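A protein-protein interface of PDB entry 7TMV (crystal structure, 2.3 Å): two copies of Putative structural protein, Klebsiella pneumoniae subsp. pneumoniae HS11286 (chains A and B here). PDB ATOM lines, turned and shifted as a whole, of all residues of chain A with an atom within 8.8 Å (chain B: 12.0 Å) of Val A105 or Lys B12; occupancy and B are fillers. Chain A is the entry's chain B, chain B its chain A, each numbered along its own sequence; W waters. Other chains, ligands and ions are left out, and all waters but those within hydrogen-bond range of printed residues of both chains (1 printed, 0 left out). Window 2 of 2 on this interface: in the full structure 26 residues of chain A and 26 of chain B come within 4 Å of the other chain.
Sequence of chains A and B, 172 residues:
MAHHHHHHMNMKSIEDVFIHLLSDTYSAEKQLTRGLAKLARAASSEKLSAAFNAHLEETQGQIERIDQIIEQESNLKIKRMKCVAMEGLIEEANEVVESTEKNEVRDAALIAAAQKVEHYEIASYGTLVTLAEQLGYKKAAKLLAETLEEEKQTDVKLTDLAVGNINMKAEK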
ATOM      1  N   SER A  44      22.928   6.484 -12.864  1.00  0.00           N
ATOM      2  CA  SER A  44      23.021   5.317 -13.766  1.00  0.00           C
ATOM      3  C   SER A  44      24.138   5.542 -14.793  1.00  0.00           C
ATOM      4  O   SER A  44      25.026   4.690 -14.874  1.00  0.00           O
ATOM      5  CB  SER A  44      21.692   5.072 -14.409  1.00  0.00           C
ATOM      6  OG  SER A  44      21.827   4.236 -15.544  1.00  0.00           O
ATOM      7  N   LEU A  48      27.077  11.143 -16.181  1.00  0.00           N
ATOM      8  CA  LEU A  48      26.541  11.960 -15.099  1.00  0.00           C
ATOM      9  C   LEU A  48      27.360  11.796 -13.824  1.00  0.00           C
ATOM     10  O   LEU A  48      27.567  12.763 -13.084  1.00  0.00           O
ATOM     11  CB  LEU A  48      25.079  11.602 -14.846  1.00  0.00           C
ATOM     12  CG  LEU A  48      24.219  12.484 -13.944  1.00  0.00           C
ATOM     13  CD1 LEU A  48      24.208  13.911 -14.369  1.00  0.00           C
ATOM     14  CD2 LEU A  48      22.788  11.916 -13.920  1.00  0.00           C
ATOM     15  N   VAL A  96      15.022  11.837  -4.845  1.00  0.00           N
ATOM     16  CA  VAL A  96      14.973  11.275  -6.187  1.00  0.00           C
ATOM     17  C   VAL A  96      15.630   9.900  -6.181  1.00  0.00           C
ATOM     18  O   VAL A  96      15.119   8.920  -6.757  1.00  0.00           O
ATOM     19  CB  VAL A  96      15.656  12.198  -7.207  1.00  0.00           C
ATOM     20  CG1 VAL A  96      15.949  11.364  -8.448  1.00  0.00           C
ATOM     21  CG2 VAL A  96      14.799  13.450  -7.563  1.00  0.00           C
ATOM     22  N   VAL A  97      16.813   9.774  -5.606  1.00  0.00           N
ATOM     23  CA  VAL A  97      17.544   8.480  -5.684  1.00  0.00           C
ATOM     24  C   VAL A  97      16.686   7.377  -5.054  1.00  0.00           C
ATOM     25  O   VAL A  97      16.722   6.260  -5.568  1.00  0.00           O
ATOM     26  CB  VAL A  97      18.928   8.582  -5.023  1.00  0.00           C
ATOM     27  CG1 VAL A  97      19.598   7.225  -4.921  1.00  0.00           C
ATOM     28  CG2 VAL A  97      19.822   9.566  -5.757  1.00  0.00           C
ATOM     29  N   SER A  99      13.331   7.191  -4.861  1.00  0.00           N
ATOM     30  CA  SER A  99      12.047   6.983  -5.545  1.00  0.00           C
ATOM     31  C   SER A  99      12.185   6.428  -6.942  1.00  0.00           C
ATOM     32  O   SER A  99      11.180   6.346  -7.650  1.00  0.00           O
ATOM     33  CB  SER A  99      11.279   8.309  -5.612  1.00  0.00           C
ATOM     34  OG  SER A  99      10.843   8.732  -4.331  1.00  0.00           O
ATOM     35  N   THR A 100      13.393   6.064  -7.363  1.00  0.00           N
ATOM     36  CA  THR A 100      13.625   5.667  -8.736  1.00  0.00           C
ATOM     37  C   THR A 100      14.556   4.473  -8.736  1.00  0.00           C
ATOM     38  O   THR A 100      15.430   4.354  -7.877  1.00  0.00           O
ATOM     39  CB  THR A 100      14.259   6.786  -9.554  1.00  0.00           C
ATOM     40  OG1 THR A 100      15.547   7.084  -9.003  1.00  0.00           O
ATOM     41  CG2 THR A 100      13.397   8.026  -9.522  1.00  0.00           C
ATOM     42  N   GLU A 101      14.388   3.622  -9.740  1.00  0.00           N
ATOM     43  CA  GLU A 101      15.371   2.610 -10.060  1.00  0.00           C
ATOM     44  C   GLU A 101      16.582   3.290 -10.675  1.00  0.00           C
ATOM     45  O   GLU A 101      16.568   4.488 -10.957  1.00  0.00           O
ATOM     46  CB  GLU A 101      14.778   1.573 -11.012  1.00  0.00           C
ATOM     47  CG  GLU A 101      13.351   1.176 -10.648  1.00  0.00           C
ATOM     48  CD  GLU A 101      13.274  -0.108  -9.828  1.00  0.00           C
ATOM     49  OE1 GLU A 101      14.326  -0.734  -9.580  1.00  0.00           O
ATOM     50  OE2 GLU A 101      12.155  -0.492  -9.417  1.00  0.00           O
ATOM     51  N   LYS A 102      17.665   2.529 -10.831  1.00  0.00           N
ATOM     52  CA  LYS A 102      18.899   3.067 -11.406  1.00  0.00           C
ATOM     53  C   LYS A 102      18.806   2.987 -12.935  1.00  0.00           C
ATOM     54  O   LYS A 102      19.492   2.209 -13.602  1.00  0.00           O
ATOM     55  CB  LYS A 102      20.114   2.317 -10.869  1.00  0.00           C
ATOM     56  CG  LYS A 102      21.372   3.178 -10.845  1.00  0.00           C
ATOM     57  CD  LYS A 102      22.515   2.600 -10.027  1.00  0.00           C
ATOM     58  CE  LYS A 102      23.847   2.880 -10.741  1.00  0.00           C
ATOM     59  NZ  LYS A 102      24.883   3.534  -9.871  1.00  0.00           N
ATOM     60  N   ASN A 103      17.974   3.860 -13.500  1.00  0.00           N
ATOM     61  CA  ASN A 103      17.697   3.850 -14.937  1.00  0.00           C
ATOM     62  C   ASN A 103      17.740   5.290 -15.449  1.00  0.00           C
ATOM     63  O   ASN A 103      18.217   6.205 -14.765  1.00  0.00           O
ATOM     64  CB  ASN A 103      16.348   3.155 -15.244  1.00  0.00           C
ATOM     65  CG  ASN A 103      15.139   3.925 -14.708  1.00  0.00           C
ATOM     66  OD1 ASN A 103      15.217   5.131 -14.531  1.00  0.00           O
ATOM     67  ND2 ASN A 103      14.013   3.237 -14.477  1.00  0.00           N
ATOM     68  N   GLU A 104      17.252   5.497 -16.668  1.00  0.00           N
ATOM     69  CA  GLU A 104      17.288   6.816 -17.283  1.00  0.00           C
ATOM     70  C   GLU A 104      16.327   7.795 -16.612  1.00  0.00           C
ATOM     71  O   GLU A 104      16.573   9.010 -16.629  1.00  0.00           O
ATOM     72  CB  GLU A 104      16.970   6.669 -18.774  1.00  0.00           C
ATOM     73  CG  GLU A 104      15.544   6.156 -19.069  1.00  0.00           C
ATOM     74  CD  GLU A 104      15.428   4.624 -19.116  1.00  0.00           C
ATOM     75  OE1 GLU A 104      16.405   3.961 -19.540  1.00  0.00           O
ATOM     76  OE2 GLU A 104      14.360   4.078 -18.726  1.00  0.00           O
ATOM     77  N   VAL A 105      15.263   7.285 -15.985  1.00  0.00           N
ATOM     78  CA  VAL A 105      14.330   8.132 -15.245  1.00  0.00           C
ATOM     79  C   VAL A 105      15.038   8.802 -14.071  1.00  0.00           C
ATOM     80  O   VAL A 105      14.933  10.024 -13.861  1.00  0.00           O
ATOM     81  CB  VAL A 105      13.124   7.293 -14.780  1.00  0.00           C
ATOM     82  CG1 VAL A 105      12.065   8.158 -14.126  1.00  0.00           C
ATOM     83  CG2 VAL A 105      12.529   6.514 -15.970  1.00  0.00           C
ATOM     84  N   ARG A 106      15.777   8.012 -13.289  1.00  0.00           N
ATOM     85  CA  ARG A 106      16.537   8.604 -12.198  1.00  0.00           C
ATOM     86  C   ARG A 106      17.495   9.665 -12.720  1.00  0.00           C
ATOM     87  O   ARG A 106      17.614  10.734 -12.118  1.00  0.00           O
ATOM     88  CB  ARG A 106      17.320   7.551 -11.420  1.00  0.00           C
ATOM     89  CG  ARG A 106      18.242   8.222 -10.399  1.00  0.00           C
ATOM     90  CD  ARG A 106      19.103   7.218  -9.616  1.00  0.00           C
ATOM     91  NE  ARG A 106      18.326   6.332  -8.759  1.00  0.00           N
ATOM     92  CZ  ARG A 106      18.832   5.289  -8.119  1.00  0.00           C
ATOM     93  NH1 ARG A 106      20.110   4.969  -8.225  1.00  0.00           N
ATOM     94  NH2 ARG A 106      18.036   4.546  -7.356  1.00  0.00           N
ATOM     95  N   ASP A 107      18.206   9.383 -13.818  1.00  0.00           N
ATOM     96  CA  ASP A 107      19.187  10.346 -14.320  1.00  0.00           C
ATOM     97  C   ASP A 107      18.487  11.646 -14.716  1.00  0.00           C
ATOM     98  O   ASP A 107      18.982  12.742 -14.418  1.00  0.00           O
ATOM     99  CB  ASP A 107      19.979   9.762 -15.503  1.00  0.00           C
ATOM    100  CG  ASP A 107      21.227   8.927 -15.058  1.00  0.00           C
ATOM    101  OD1 ASP A 107      21.710   9.071 -13.901  1.00  0.00           O
ATOM    102  OD2 ASP A 107      21.716   8.091 -15.861  1.00  0.00           O
ATOM    103  N   ALA A 108      17.299  11.563 -15.326  1.00  0.00           N
ATOM    104  CA  ALA A 108      16.606  12.812 -15.667  1.00  0.00           C
ATOM    105  C   ALA A 108      16.297  13.620 -14.418  1.00  0.00           C
ATOM    106  O   ALA A 108      16.570  14.834 -14.353  1.00  0.00           O
ATOM    107  CB  ALA A 108      15.310  12.542 -16.424  1.00  0.00           C
ATOM    108  N   ALA A 109      15.713  12.955 -13.404  1.00  0.00           N
ATOM    109  CA  ALA A 109      15.262  13.696 -12.222  1.00  0.00           C
ATOM    110  C   ALA A 109      16.439  14.195 -11.380  1.00  0.00           C
ATOM    111  O   ALA A 109      16.331  15.216 -10.680  1.00  0.00           O
ATOM    112  CB  ALA A 109      14.315  12.822 -11.407  1.00  0.00           C
ATOM    113  N   LEU A 110      17.559  13.470 -11.422  1.00  0.00           N
ATOM    114  CA  LEU A 110      18.765  13.855 -10.698  1.00  0.00           C
ATOM    115  C   LEU A 110      19.449  15.036 -11.363  1.00  0.00           C
ATOM    116  O   LEU A 110      19.918  15.954 -10.678  1.00  0.00           O
ATOM    117  CB  LEU A 110      19.704  12.653 -10.618  1.00  0.00           C
ATOM    118  CG  LEU A 110      20.315  12.324  -9.257  1.00  0.00           C
ATOM    119  CD1 LEU A 110      19.270  11.983  -8.238  1.00  0.00           C
ATOM    120  CD2 LEU A 110      21.298  11.158  -9.398  1.00  0.00           C
ATOM    121  N   ILE A 111      19.517  15.036 -12.696  1.00  0.00           N
ATOM    122  CA  ILE A 111      19.986  16.222 -13.402  1.00  0.00           C
ATOM    123  C   ILE A 111      19.137  17.419 -12.996  1.00  0.00           C
ATOM    124  O   ILE A 111      19.660  18.478 -12.623  1.00  0.00           O
ATOM    125  CB  ILE A 111      19.936  15.998 -14.923  1.00  0.00           C
ATOM    126  CG1 ILE A 111      21.153  15.201 -15.376  1.00  0.00           C
ATOM    127  CG2 ILE A 111      19.873  17.338 -15.674  1.00  0.00           C
ATOM    128  CD1 ILE A 111      21.049  14.668 -16.778  1.00  0.00           C
ATOM    129  N   ALA A 112      17.811  17.239 -12.997  1.00  0.00           N
ATOM    130  CA  ALA A 112      16.917  18.346 -12.635  1.00  0.00           C
ATOM    131  C   ALA A 112      17.227  18.888 -11.238  1.00  0.00           C
ATOM    132  O   ALA A 112      17.297  20.116 -11.028  1.00  0.00           O
ATOM    133  CB  ALA A 112      15.458  17.885 -12.714  1.00  0.00           C
ATOM    134  N   MET B  11       8.504   7.327  -8.955  1.00  0.00           N
ATOM    135  CA  MET B  11       8.464   7.837 -10.318  1.00  0.00           C
ATOM    136  C   MET B  11       9.045   6.781 -11.250  1.00  0.00           C
ATOM    137  O   MET B  11      10.267   6.599 -11.302  1.00  0.00           O
ATOM    138  CB  MET B  11       9.243   9.142 -10.405  1.00  0.00           C
ATOM    139  CG  MET B  11       8.417  10.329  -9.985  1.00  0.00           C
ATOM    140  SD  MET B  11       9.347  11.854  -9.721  1.00  0.00           S
ATOM    141  CE  MET B  11      10.986  11.274  -9.313  1.00  0.00           C
ATOM    142  N   LYS B  12       8.178   6.146 -12.045  1.00  0.00           N
ATOM    143  CA  LYS B  12       8.586   5.028 -12.885  1.00  0.00           C
ATOM    144  C   LYS B  12       8.765   5.404 -14.350  1.00  0.00           C
ATOM    145  O   LYS B  12       9.340   4.608 -15.100  1.00  0.00           O
ATOM    146  CB  LYS B  12       7.576   3.866 -12.788  1.00  0.00           C
ATOM    147  N   SER B  13       8.306   6.580 -14.784  1.00  0.00           N
ATOM    148  CA  SER B  13       8.512   6.987 -16.170  1.00  0.00           C
ATOM    149  C   SER B  13       8.899   8.458 -16.250  1.00  0.00           C
ATOM    150  O   SER B  13       8.798   9.214 -15.283  1.00  0.00           O
ATOM    151  CB  SER B  13       7.272   6.787 -17.036  1.00  0.00           C
ATOM    152  OG  SER B  13       6.269   7.710 -16.652  1.00  0.00           O
ATOM    153  N   ILE B  14       9.332   8.869 -17.441  1.00  0.00           N
ATOM    154  CA  ILE B  14       9.605  10.283 -17.684  1.00  0.00           C
ATOM    155  C   ILE B  14       8.330  11.116 -17.570  1.00  0.00           C
ATOM    156  O   ILE B  14       8.357  12.233 -17.052  1.00  0.00           O
ATOM    157  CB  ILE B  14      10.275  10.459 -19.055  1.00  0.00           C
ATOM    158  CG1 ILE B  14      11.614   9.713 -19.107  1.00  0.00           C
ATOM    159  CG2 ILE B  14      10.507  11.916 -19.349  1.00  0.00           C
ATOM    160  CD1 ILE B  14      12.605  10.135 -18.068  1.00  0.00           C
ATOM    161  N   GLU B  15       7.188  10.595 -18.021  1.00  0.00           N
ATOM    162  CA  GLU B  15       5.957  11.362 -17.841  1.00  0.00           C
ATOM    163  C   GLU B  15       5.711  11.659 -16.364  1.00  0.00           C
ATOM    164  O   GLU B  15       5.264  12.761 -16.011  1.00  0.00           O
ATOM    165  CB  GLU B  15       4.744  10.636 -18.413  1.00  0.00           C
ATOM    166  CG  GLU B  15       4.926   9.989 -19.754  1.00  0.00           C
ATOM    167  CD  GLU B  15       3.729  10.193 -20.657  1.00  0.00           C
ATOM    168  OE1 GLU B  15       3.113  11.287 -20.611  1.00  0.00           O
ATOM    169  OE2 GLU B  15       3.421   9.255 -21.426  1.00  0.00           O
ATOM    170  N   ASP B  16       5.956  10.671 -15.486  1.00  0.00           N
ATOM    171  CA  ASP B  16       5.768  10.888 -14.048  1.00  0.00           C
ATOM    172  C   ASP B  16       6.682  11.990 -13.530  1.00  0.00           C
ATOM    173  O   ASP B  16       6.248  12.852 -12.764  1.00  0.00           O
ATOM    174  CB  ASP B  16       5.983   9.589 -13.282  1.00  0.00           C
ATOM    175  CG  ASP B  16       4.846   8.620 -13.483  1.00  0.00           C
ATOM    176  OD1 ASP B  16       3.687   9.092 -13.559  1.00  0.00           O
ATOM    177  OD2 ASP B  16       5.108   7.400 -13.593  1.00  0.00           O
ATOM    178  N   VAL B  17       7.939  12.003 -13.959  1.00  0.00           N
ATOM    179  CA  VAL B  17       8.820  13.087 -13.547  1.00  0.00           C
ATOM    180  C   VAL B  17       8.264  14.422 -14.046  1.00  0.00           C
ATOM    181  O   VAL B  17       8.252  15.426 -13.319  1.00  0.00           O
ATOM    182  CB  VAL B  17      10.248  12.827 -14.062  1.00  0.00           C
ATOM    183  CG1 VAL B  17      11.108  14.085 -13.905  1.00  0.00           C
ATOM    184  CG2 VAL B  17      10.843  11.648 -13.319  1.00  0.00           C
ATOM    185  N   PHE B  18       7.768  14.439 -15.283  1.00  0.00           N
ATOM    186  CA  PHE B  18       7.232  15.666 -15.857  1.00  0.00           C
ATOM    187  C   PHE B  18       6.062  16.166 -15.027  1.00  0.00           C
ATOM    188  O   PHE B  18       6.038  17.323 -14.614  1.00  0.00           O
ATOM    189  CB  PHE B  18       6.820  15.395 -17.317  1.00  0.00           C
ATOM    190  CG  PHE B  18       6.220  16.574 -18.025  1.00  0.00           C
ATOM    191  CD1 PHE B  18       6.987  17.671 -18.345  1.00  0.00           C
ATOM    192  CD2 PHE B  18       4.887  16.569 -18.394  1.00  0.00           C
ATOM    193  CE1 PHE B  18       6.432  18.759 -19.018  1.00  0.00           C
ATOM    194  CE2 PHE B  18       4.318  17.664 -19.050  1.00  0.00           C
ATOM    195  CZ  PHE B  18       5.098  18.754 -19.367  1.00  0.00           C
ATOM    196  N   ILE B  19       5.120  15.285 -14.710  1.00  0.00           N
ATOM    197  CA  ILE B  19       3.922  15.701 -13.985  1.00  0.00           C
ATOM    198  C   ILE B  19       4.268  16.102 -12.545  1.00  0.00           C
ATOM    199  O   ILE B  19       3.692  17.047 -11.981  1.00  0.00           O
ATOM    200  CB  ILE B  19       2.866  14.584 -14.068  1.00  0.00           C
ATOM    201  CG1 ILE B  19       1.462  15.127 -13.788  1.00  0.00           C
ATOM    202  CG2 ILE B  19       3.184  13.462 -13.114  1.00  0.00           C
ATOM    203  CD1 ILE B  19       1.090  16.425 -14.546  1.00  0.00           C
ATOM    204  N   HIS B  20       5.224  15.415 -11.932  1.00  0.00           N
ATOM    205  CA  HIS B  20       5.631  15.801 -10.585  1.00  0.00           C
ATOM    206  C   HIS B  20       6.256  17.192 -10.582  1.00  0.00           C
ATOM    207  O   HIS B  20       5.925  18.035  -9.735  1.00  0.00           O
ATOM    208  CB  HIS B  20       6.604  14.773 -10.008  1.00  0.00           C
ATOM    209  CG  HIS B  20       7.187  15.189  -8.699  1.00  0.00           C
ATOM    210  ND1 HIS B  20       6.528  15.002  -7.502  1.00  0.00           N
ATOM    211  CD2 HIS B  20       8.345  15.823  -8.398  1.00  0.00           C
ATOM    212  CE1 HIS B  20       7.260  15.493  -6.518  1.00  0.00           C
ATOM    213  NE2 HIS B  20       8.372  15.989  -7.033  1.00  0.00           N
ATOM    214  N   LEU B  21       7.170  17.458 -11.517  1.00  0.00           N
ATOM    215  CA  LEU B  21       7.788  18.780 -11.546  1.00  0.00           C
ATOM    216  C   LEU B  21       6.781  19.853 -11.934  1.00  0.00           C
ATOM    217  O   LEU B  21       6.850  20.986 -11.447  1.00  0.00           O
ATOM    218  CB  LEU B  21       8.967  18.786 -12.506  1.00  0.00           C
ATOM    219  CG  LEU B  21      10.214  18.050 -12.003  1.00  0.00           C
ATOM    220  CD1 LEU B  21      11.340  18.387 -13.038  1.00  0.00           C
ATOM    221  CD2 LEU B  21      10.644  18.397 -10.600  1.00  0.00           C
ATOM    222  N   THR B 127      14.165  22.518 -17.070  1.00  0.00           N
ATOM    223  CA  THR B 127      13.919  21.080 -17.065  1.00  0.00           C
ATOM    224  C   THR B 127      12.594  20.759 -17.742  1.00  0.00           C
ATOM    225  O   THR B 127      12.511  19.820 -18.542  1.00  0.00           O
ATOM    226  CB  THR B 127      13.908  20.534 -15.638  1.00  0.00           C
ATOM    227  OG1 THR B 127      15.184  20.731 -15.017  1.00  0.00           O
ATOM    228  CG2 THR B 127      13.590  19.036 -15.665  1.00  0.00           C
ATOM    229  N   THR B 130      12.953  20.937 -21.507  1.00  0.00           N
ATOM    230  CA  THR B 130      13.681  19.792 -22.041  1.00  0.00           C
ATOM    231  C   THR B 130      12.768  18.583 -22.113  1.00  0.00           C
ATOM    232  O   THR B 130      12.735  17.860 -23.117  1.00  0.00           O
ATOM    233  CB  THR B 130      14.904  19.469 -21.171  1.00  0.00           C
ATOM    234  OG1 THR B 130      15.851  20.550 -21.224  1.00  0.00           O
ATOM    235  CG2 THR B 130      15.564  18.149 -21.638  1.00  0.00           C
ATOM    236  N   LEU B 131      12.025  18.340 -21.035  1.00  0.00           N
ATOM    237  CA  LEU B 131      11.245  17.110 -20.937  1.00  0.00           C
ATOM    238  C   LEU B 131      10.003  17.146 -21.816  1.00  0.00           C
ATOM    239  O   LEU B 131       9.635  16.114 -22.407  1.00  0.00           O
ATOM    240  CB  LEU B 131      10.864  16.852 -19.491  1.00  0.00           C
ATOM    241  CG  LEU B 131      12.042  16.518 -18.575  1.00  0.00           C
ATOM    242  CD1 LEU B 131      11.418  16.236 -17.181  1.00  0.00           C
ATOM    243  CD2 LEU B 131      12.909  15.363 -18.989  1.00  0.00           C
ATOM    244  N   GLN B 134      10.665  16.068 -25.192  1.00  0.00           N
ATOM    245  CA  GLN B 134      10.755  14.617 -25.334  1.00  0.00           C
ATOM    246  C   GLN B 134       9.374  13.969 -25.377  1.00  0.00           C
ATOM    247  O   GLN B 134       9.130  13.059 -26.176  1.00  0.00           O
ATOM    248  CB  GLN B 134      11.577  14.039 -24.182  1.00  0.00           C
ATOM    249  CG  GLN B 134      13.060  13.860 -24.531  1.00  0.00           C
ATOM    250  CD  GLN B 134      13.972  13.991 -23.314  1.00  0.00           C
ATOM    251  OE1 GLN B 134      15.018  14.650 -23.379  1.00  0.00           O
ATOM    252  NE2 GLN B 134      13.575  13.372 -22.195  1.00  0.00           N
ATOM    253  N   LEU B 135       8.442  14.434 -24.550  1.00  0.00           N
ATOM    254  CA  LEU B 135       7.145  13.761 -24.483  1.00  0.00           C
ATOM    255  C   LEU B 135       6.173  14.129 -25.605  1.00  0.00           C
ATOM    256  O   LEU B 135       5.071  13.564 -25.650  1.00  0.00           O
ATOM    257  CB  LEU B 135       6.481  14.049 -23.140  1.00  0.00           C
ATOM    258  CG  LEU B 135       6.806  13.052 -22.031  1.00  0.00           C
ATOM    259  CD1 LEU B 135       8.260  13.189 -21.640  1.00  0.00           C
ATOM    260  CD2 LEU B 135       5.893  13.254 -20.820  1.00  0.00           C
HETATM  261  O   HOH W   1      15.702  21.758 -12.577  1.00  0.00           O
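Water W1 lies within hydrogen-bond range of the side-chain hydroxyl (OG1) of Thr B127 and the backbone carbonyl oxygen (O) of Ala A112.
Of chain B, only Ile B14 (3.98 Å) comes within 4 Å of Ala A108. No residue of chain B comes within 4 Å of Ala A109. Ser B13 touches one residue of chain A. Printed residues of chain B within 4 Å of Ala A112: Thr B127 (3.7 Å). Of the printed residues of chain A, Thr B127 touches Ala A112. Of the printed residues of chain A, Ile B14 touches Val A105 and Ala A108. Of the printed residues of chain A, Val B17 touches Val A105 (3.8 Å). Of the printed residues of chain B, Ser A99 touches Met B11 (3.1 Å). The nearest residue of chain A that does not touch Lys B12 is Asn A103 (4.9 Å).
No position is printed for both chains. Of the 9 pairs that touch across the chains among the printed residues, none has its exchanged pair printed and touching as well.
The side-chain hydroxyl (OG) of Ser B13 lies close to the backbone NH (N) of Glu B15 (3.3 Å). N of Asp B16 is in hydrogen-bond range of OG of Ser B13 (3.2 Å). The backbone carbonyl oxygen (O) of Val A96 lies within hydrogen-bond range of the side-chain hydroxyl (OG1) of Thr A100 (2.9 Å). The backbone carbonyl oxygen of Thr A100 lies within hydrogen-bond range of the guanidinium group of Arg A106 (2.7 Å). The backbone NH (N) of Val A105 sits at hydrogen-bond distance from the side-chain amide oxygen (OD1) of Asn A103.
The backbone NH of Met B11 sits at hydrogen-bond distance from the backbone carbonyl oxygen of Ser A99, 3.1 Å away.
Among the printed residues, merely in contact across the chains: Val A105 with Ser B13, Ala A112 with Thr B127, Val A105 with Met B11, Val A105 with Val B17, Val A105 with Lys B12, Val A105 with Ile B14, Thr A100 with Met B11 and Ala A108 with Ile B14.
Of the 16 printed residues of chain B, 6 touch a printed residue of chain A. Hydrophobic or aromatic side chains of chain B that line the printed part of chain A: Ile B14 and Val B17. Along chain B the printed residues that touch a printed residue of chain A span positions 11 to 127. Of the 18 printed residues of chain A, 5 touch a printed residue of chain B. Hydrophobic or aromatic side chains of chain A within 4 Å of the printed part of chain B: Val A105, Ala A108 and Ala A112. Among the printed residues, 9 pairs touch across the chains. Among the printed residues, no Asp or Glu carboxylate lies within 4 Å of a Lys or Arg side-chain nitrogen of the other chain.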
